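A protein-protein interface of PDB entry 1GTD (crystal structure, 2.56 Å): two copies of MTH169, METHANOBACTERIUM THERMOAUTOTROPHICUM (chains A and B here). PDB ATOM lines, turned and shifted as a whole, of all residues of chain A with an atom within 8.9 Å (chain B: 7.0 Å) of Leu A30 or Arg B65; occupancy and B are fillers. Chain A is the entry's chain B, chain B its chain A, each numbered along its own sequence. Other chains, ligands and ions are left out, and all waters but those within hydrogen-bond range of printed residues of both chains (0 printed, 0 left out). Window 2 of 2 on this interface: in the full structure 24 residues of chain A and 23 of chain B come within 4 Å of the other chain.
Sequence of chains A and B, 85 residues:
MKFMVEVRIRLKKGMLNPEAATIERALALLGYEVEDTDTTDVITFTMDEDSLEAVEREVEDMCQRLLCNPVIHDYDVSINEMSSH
OD2 of Asp B61 is in hydrogen-bond range of OH of Tyr A32, 2.6 Å away.
The guanidinium group (NH1) of Arg B65 is in salt-bridge range of the side-chain carboxylate (OD2) of Asp B61, at 3.2 Å.
The backbone carbonyl oxygen (O) of Met B62 is in hydrogen-bond range of the backbone NH (N) of Leu B67 (2.9 Å).
The backbone NH (N) of Tyr A32 lies within hydrogen-bond range of the backbone carbonyl oxygen (O) of Leu A27 (3.0 Å).
Leu B67 touches Ile A23 (CD2 to CG2, 3.9 Å).
Leu A27 touches Met B62 (CD2 to CG, 3.98 Å).
CD2 of Leu A27 touches CG of Leu B66, 3.95 Å away.
Leu A30 touches Arg B65.
CE of Met B62 touches CG of Tyr A32, at 3.3 Å.
Of the printed residues of chain B, Ile A23 touches Leu B67.
Of the printed residues of chain B, Leu A27 touches Met B62 and Leu B66.
Gly A31 touches none of the printed residues of chain B.
Printed residues of chain B within 4 Å of Tyr A32: Asp B61 and Met B62.
Of chain A, only Leu A30 (3.1 Å) comes within 4 Å of Arg B65.
Of the printed residues of chain A, Leu B67 touches Ile A23 (3.9 Å).
Cys B68 touches none of the printed residues of chain A.
The nearest printed residue of chain B that does not touch Tyr A32 is Arg B65 (4.1 Å).
Of the 11 printed residues of chain B, 5 touch a printed residue of chain A.
Printed residues of chain B that touch a printed residue of chain A: Asp B61, Met B62, Arg B65, Leu B66 and Leu B67.
Hydrophobic or aromatic side chains of chain B within 4 Å of the printed part of chain A: Met B62, Leu B66 and Leu B67.
Printed residues of chain A that touch a printed residue of chain B: Ile A23, Leu A27, Leu A30 and Tyr A32.
Hydrophobic or aromatic side chains of chain A that line the printed part of chain B: Ile A23, Leu A27, Leu A30 and Tyr A32.
Among the printed residues, 6 pairs touch across the chains.
Among the printed residues, no Asp or Glu carboxylate lies within 4 Å of a Lys or Arg side-chain nitrogen of the other chain.
No position is printed for both chains.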
ATOM      1  N   ILE A  23       4.554  21.836 -11.644  1.00  0.00           N
ATOM      2  CA  ILE A  23       5.356  20.662 -11.939  1.00  0.00           C
ATOM      3  C   ILE A  23       4.893  19.997 -13.233  1.00  0.00           C
ATOM      4  O   ILE A  23       5.689  19.736 -14.133  1.00  0.00           O
ATOM      5  CB  ILE A  23       5.245  19.638 -10.810  1.00  0.00           C
ATOM      6  CG1 ILE A  23       5.940  20.160  -9.551  1.00  0.00           C
ATOM      7  CG2 ILE A  23       5.831  18.326 -11.247  1.00  0.00           C
ATOM      8  CD1 ILE A  23       5.794  19.239  -8.351  1.00  0.00           C
ATOM      9  N   GLU A  24       3.599  19.727 -13.321  1.00  0.00           N
ATOM     10  CA  GLU A  24       3.032  19.068 -14.490  1.00  0.00           C
ATOM     11  C   GLU A  24       3.357  19.788 -15.785  1.00  0.00           C
ATOM     12  O   GLU A  24       3.805  19.167 -16.749  1.00  0.00           O
ATOM     13  CB  GLU A  24       1.515  18.945 -14.336  1.00  0.00           C
ATOM     14  CG  GLU A  24       0.857  18.139 -15.433  1.00  0.00           C
ATOM     15  CD  GLU A  24      -0.577  17.760 -15.101  1.00  0.00           C
ATOM     16  OE1 GLU A  24      -0.799  17.113 -14.052  1.00  0.00           O
ATOM     17  OE2 GLU A  24      -1.482  18.104 -15.895  1.00  0.00           O
ATOM     18  N   ARG A  25       3.127  21.095 -15.812  1.00  0.00           N
ATOM     19  CA  ARG A  25       3.406  21.884 -17.003  1.00  0.00           C
ATOM     20  C   ARG A  25       4.883  21.833 -17.375  1.00  0.00           C
ATOM     21  O   ARG A  25       5.235  21.651 -18.545  1.00  0.00           O
ATOM     22  CB  ARG A  25       2.990  23.338 -16.788  1.00  0.00           C
ATOM     23  CG  ARG A  25       3.544  24.287 -17.844  1.00  0.00           C
ATOM     24  CD  ARG A  25       2.761  25.592 -17.906  1.00  0.00           C
ATOM     25  NE  ARG A  25       3.250  26.442 -18.989  1.00  0.00           N
ATOM     26  CZ  ARG A  25       4.403  27.102 -18.951  1.00  0.00           C
ATOM     27  NH1 ARG A  25       5.182  27.014 -17.880  1.00  0.00           N
ATOM     28  NH2 ARG A  25       4.783  27.844 -19.981  1.00  0.00           N
ATOM     29  N   ALA A  26       5.743  22.003 -16.376  1.00  0.00           N
ATOM     30  CA  ALA A  26       7.179  21.984 -16.594  1.00  0.00           C
ATOM     31  C   ALA A  26       7.592  20.638 -17.155  1.00  0.00           C
ATOM     32  O   ALA A  26       8.427  20.571 -18.055  1.00  0.00           O
ATOM     33  CB  ALA A  26       7.907  22.255 -15.288  1.00  0.00           C
ATOM     34  N   LEU A  27       7.008  19.563 -16.627  1.00  0.00           N
ATOM     35  CA  LEU A  27       7.339  18.227 -17.115  1.00  0.00           C
ATOM     36  C   LEU A  27       6.931  18.097 -18.578  1.00  0.00           C
ATOM     37  O   LEU A  27       7.711  17.649 -19.411  1.00  0.00           O
ATOM     38  CB  LEU A  27       6.650  17.141 -16.266  1.00  0.00           C
ATOM     39  CG  LEU A  27       7.158  16.978 -14.817  1.00  0.00           C
ATOM     40  CD1 LEU A  27       6.479  15.786 -14.141  1.00  0.00           C
ATOM     41  CD2 LEU A  27       8.683  16.793 -14.815  1.00  0.00           C
ATOM     42  N   ALA A  28       5.704  18.494 -18.894  1.00  0.00           N
ATOM     43  CA  ALA A  28       5.218  18.422 -20.266  1.00  0.00           C
ATOM     44  C   ALA A  28       6.212  19.097 -21.205  1.00  0.00           C
ATOM     45  O   ALA A  28       6.561  18.548 -22.248  1.00  0.00           O
ATOM     46  CB  ALA A  28       3.854  19.095 -20.373  1.00  0.00           C
ATOM     47  N   LEU A  29       6.674  20.285 -20.824  1.00  0.00           N
ATOM     48  CA  LEU A  29       7.626  21.037 -21.637  1.00  0.00           C
ATOM     49  C   LEU A  29       8.970  20.320 -21.792  1.00  0.00           C
ATOM     50  O   LEU A  29       9.610  20.381 -22.845  1.00  0.00           O
ATOM     51  CB  LEU A  29       7.861  22.412 -21.015  1.00  0.00           C
ATOM     52  CG  LEU A  29       6.665  23.346 -20.943  1.00  0.00           C
ATOM     53  CD1 LEU A  29       7.030  24.552 -20.122  1.00  0.00           C
ATOM     54  CD2 LEU A  29       6.259  23.755 -22.341  1.00  0.00           C
ATOM     55  N   LEU A  30       9.394  19.652 -20.728  1.00  0.00           N
ATOM     56  CA  LEU A  30      10.652  18.924 -20.726  1.00  0.00           C
ATOM     57  C   LEU A  30      10.553  17.640 -21.549  1.00  0.00           C
ATOM     58  O   LEU A  30      11.545  16.936 -21.732  1.00  0.00           O
ATOM     59  CB  LEU A  30      11.040  18.577 -19.291  1.00  0.00           C
ATOM     60  CG  LEU A  30      12.521  18.604 -18.900  1.00  0.00           C
ATOM     61  CD1 LEU A  30      13.082  20.036 -19.018  1.00  0.00           C
ATOM     62  CD2 LEU A  30      12.664  18.083 -17.469  1.00  0.00           C
ATOM     63  N   GLY A  31       9.355  17.326 -22.032  1.00  0.00           N
ATOM     64  CA  GLY A  31       9.182  16.130 -22.836  1.00  0.00           C
ATOM     65  C   GLY A  31       8.295  15.068 -22.227  1.00  0.00           C
ATOM     66  O   GLY A  31       7.735  14.244 -22.942  1.00  0.00           O
ATOM     67  N   TYR A  32       8.156  15.092 -20.906  1.00  0.00           N
ATOM     68  CA  TYR A  32       7.344  14.108 -20.190  1.00  0.00           C
ATOM     69  C   TYR A  32       5.902  14.556 -20.026  1.00  0.00           C
ATOM     70  O   TYR A  32       5.643  15.716 -19.717  1.00  0.00           O
ATOM     71  CB  TYR A  32       7.947  13.852 -18.811  1.00  0.00           C
ATOM     72  CG  TYR A  32       9.411  13.526 -18.870  1.00  0.00           C
ATOM     73  CD1 TYR A  32      10.344  14.295 -18.184  1.00  0.00           C
ATOM     74  CD2 TYR A  32       9.870  12.467 -19.643  1.00  0.00           C
ATOM     75  CE1 TYR A  32      11.700  14.020 -18.268  1.00  0.00           C
ATOM     76  CE2 TYR A  32      11.221  12.183 -19.738  1.00  0.00           C
ATOM     77  CZ  TYR A  32      12.133  12.961 -19.051  1.00  0.00           C
ATOM     78  OH  TYR A  32      13.477  12.674 -19.157  1.00  0.00           O
ATOM     79  N   GLU A  33       4.966  13.631 -20.219  1.00  0.00           N
ATOM     80  CA  GLU A  33       3.552  13.958 -20.084  1.00  0.00           C
ATOM     81  C   GLU A  33       2.918  13.173 -18.944  1.00  0.00           C
ATOM     82  O   GLU A  33       2.684  11.969 -19.049  1.00  0.00           O
ATOM     83  CB  GLU A  33       2.803  13.657 -21.382  1.00  0.00           C
ATOM     84  CG  GLU A  33       1.456  14.347 -21.459  1.00  0.00           C
ATOM     85  CD  GLU A  33       1.596  15.844 -21.687  1.00  0.00           C
ATOM     86  OE1 GLU A  33       0.827  16.621 -21.068  1.00  0.00           O
ATOM     87  OE2 GLU A  33       2.473  16.241 -22.494  1.00  0.00           O
ATOM     88  N   VAL B  59      11.101   8.598 -14.865  1.00  0.00           N
ATOM     89  CA  VAL B  59      10.851   9.233 -13.580  1.00  0.00           C
ATOM     90  C   VAL B  59      12.197   9.623 -12.987  1.00  0.00           C
ATOM     91  O   VAL B  59      12.365  10.733 -12.494  1.00  0.00           O
ATOM     92  CB  VAL B  59      10.115   8.297 -12.601  1.00  0.00           C
ATOM     93  CG1 VAL B  59       9.964   8.974 -11.244  1.00  0.00           C
ATOM     94  CG2 VAL B  59       8.755   7.953 -13.150  1.00  0.00           C
ATOM     95  N   GLU B  60      13.155   8.704 -13.054  1.00  0.00           N
ATOM     96  CA  GLU B  60      14.499   8.931 -12.533  1.00  0.00           C
ATOM     97  C   GLU B  60      15.104  10.188 -13.139  1.00  0.00           C
ATOM     98  O   GLU B  60      15.832  10.921 -12.479  1.00  0.00           O
ATOM     99  CB  GLU B  60      15.380   7.720 -12.844  1.00  0.00           C
ATOM    100  CG  GLU B  60      16.883   7.971 -12.756  1.00  0.00           C
ATOM    101  CD  GLU B  60      17.332   8.364 -11.366  1.00  0.00           C
ATOM    102  OE1 GLU B  60      18.560   8.513 -11.154  1.00  0.00           O
ATOM    103  OE2 GLU B  60      16.455   8.522 -10.487  1.00  0.00           O
ATOM    104  N   ASP B  61      14.791  10.442 -14.401  1.00  0.00           N
ATOM    105  CA  ASP B  61      15.311  11.615 -15.085  1.00  0.00           C
ATOM    106  C   ASP B  61      14.657  12.873 -14.523  1.00  0.00           C
ATOM    107  O   ASP B  61      15.330  13.872 -14.273  1.00  0.00           O
ATOM    108  CB  ASP B  61      15.027  11.511 -16.579  1.00  0.00           C
ATOM    109  CG  ASP B  61      16.085  12.178 -17.410  1.00  0.00           C
ATOM    110  OD1 ASP B  61      17.239  11.696 -17.382  1.00  0.00           O
ATOM    111  OD2 ASP B  61      15.773  13.181 -18.087  1.00  0.00           O
ATOM    112  N   MET B  62      13.341  12.815 -14.325  1.00  0.00           N
ATOM    113  CA  MET B  62      12.578  13.942 -13.787  1.00  0.00           C
ATOM    114  C   MET B  62      13.089  14.354 -12.414  1.00  0.00           C
ATOM    115  O   MET B  62      13.134  15.541 -12.086  1.00  0.00           O
ATOM    116  CB  MET B  62      11.098  13.576 -13.681  1.00  0.00           C
ATOM    117  CG  MET B  62      10.447  13.235 -15.008  1.00  0.00           C
ATOM    118  SD  MET B  62       8.675  12.500 -14.789  1.00  0.00           S
ATOM    119  CE  MET B  62       8.543  11.475 -16.434  1.00  0.00           C
ATOM    120  N   CYS B  63      13.463  13.370 -11.609  1.00  0.00           N
ATOM    121  CA  CYS B  63      13.978  13.644 -10.280  1.00  0.00           C
ATOM    122  C   CYS B  63      15.346  14.298 -10.366  1.00  0.00           C
ATOM    123  O   CYS B  63      15.649  15.214  -9.604  1.00  0.00           O
ATOM    124  CB  CYS B  63      14.093  12.352  -9.482  1.00  0.00           C
ATOM    125  SG  CYS B  63      12.531  11.524  -9.271  1.00  0.00           S
ATOM    126  N   GLN B  64      16.167  13.822 -11.295  1.00  0.00           N
ATOM    127  CA  GLN B  64      17.513  14.350 -11.476  1.00  0.00           C
ATOM    128  C   GLN B  64      17.559  15.790 -11.987  1.00  0.00           C
ATOM    129  O   GLN B  64      18.421  16.569 -11.575  1.00  0.00           O
ATOM    130  CB  GLN B  64      18.297  13.464 -12.447  1.00  0.00           C
ATOM    131  CG  GLN B  64      18.482  12.036 -11.975  1.00  0.00           C
ATOM    132  CD  GLN B  64      19.472  11.923 -10.839  1.00  0.00           C
ATOM    133  OE1 GLN B  64      19.625  10.858 -10.233  1.00  0.00           O
ATOM    134  NE2 GLN B  64      20.164  13.023 -10.548  1.00  0.00           N
ATOM    135  N   ARG B  65      16.633  16.146 -12.875  1.00  0.00           N
ATOM    136  CA  ARG B  65      16.639  17.483 -13.455  1.00  0.00           C
ATOM    137  C   ARG B  65      15.434  18.372 -13.195  1.00  0.00           C
ATOM    138  O   ARG B  65      15.253  19.372 -13.893  1.00  0.00           O
ATOM    139  CB  ARG B  65      16.862  17.385 -14.972  1.00  0.00           C
ATOM    140  CG  ARG B  65      15.998  16.344 -15.659  1.00  0.00           C
ATOM    141  CD  ARG B  65      16.397  16.097 -17.122  1.00  0.00           C
ATOM    142  NE  ARG B  65      15.894  17.122 -18.040  1.00  0.00           N
ATOM    143  CZ  ARG B  65      15.733  16.949 -19.353  1.00  0.00           C
ATOM    144  NH1 ARG B  65      16.032  15.788 -19.928  1.00  0.00           N
ATOM    145  NH2 ARG B  65      15.269  17.943 -20.101  1.00  0.00           N
ATOM    146  N   LEU B  66      14.619  18.056 -12.195  1.00  0.00           N
ATOM    147  CA  LEU B  66      13.449  18.895 -11.963  1.00  0.00           C
ATOM    148  C   LEU B  66      12.834  18.787 -10.572  1.00  0.00           C
ATOM    149  O   LEU B  66      12.714  19.788  -9.863  1.00  0.00           O
ATOM    150  CB  LEU B  66      12.390  18.584 -13.038  1.00  0.00           C
ATOM    151  CG  LEU B  66      11.179  19.485 -13.352  1.00  0.00           C
ATOM    152  CD1 LEU B  66      10.167  19.442 -12.226  1.00  0.00           C
ATOM    153  CD2 LEU B  66      11.633  20.907 -13.599  1.00  0.00           C
ATOM    154  N   LEU B  67      12.455  17.576 -10.180  1.00  0.00           N
ATOM    155  CA  LEU B  67      11.800  17.374  -8.891  1.00  0.00           C
ATOM    156  C   LEU B  67      12.629  17.631  -7.629  1.00  0.00           C
ATOM    157  O   LEU B  67      12.090  18.064  -6.607  1.00  0.00           O
ATOM    158  CB  LEU B  67      11.183  15.972  -8.839  1.00  0.00           C
ATOM    159  CG  LEU B  67      10.199  15.662  -9.977  1.00  0.00           C
ATOM    160  CD1 LEU B  67       9.437  14.389  -9.653  1.00  0.00           C
ATOM    161  CD2 LEU B  67       9.217  16.818 -10.166  1.00  0.00           C
ATOM    162  N   CYS B  68      13.927  17.379  -7.678  1.00  0.00           N
ATOM    163  CA  CYS B  68      14.733  17.617  -6.491  1.00  0.00           C
ATOM    164  C   CYS B  68      16.212  17.796  -6.799  1.00  0.00           C
ATOM    165  O   CYS B  68      16.633  17.764  -7.966  1.00  0.00           O
ATOM    166  CB  CYS B  68      14.562  16.461  -5.505  1.00  0.00           C
ATOM    167  SG  CYS B  68      15.347  14.935  -6.051  1.00  0.00           S
ATOM    168  N   PRO B  70      19.435  15.931  -5.846  1.00  0.00           N
ATOM    169  CA  PRO B  70      20.037  14.756  -5.212  1.00  0.00           C
ATOM    170  C   PRO B  70      21.217  15.072  -4.298  1.00  0.00           C
ATOM    171  O   PRO B  70      21.499  14.337  -3.350  1.00  0.00           O
ATOM    172  CB  PRO B  70      20.419  13.875  -6.400  1.00  0.00           C
ATOM    173  CG  PRO B  70      20.452  14.822  -7.568  1.00  0.00           C
ATOM    174  CD  PRO B  70      19.311  15.737  -7.297  1.00  0.00           C
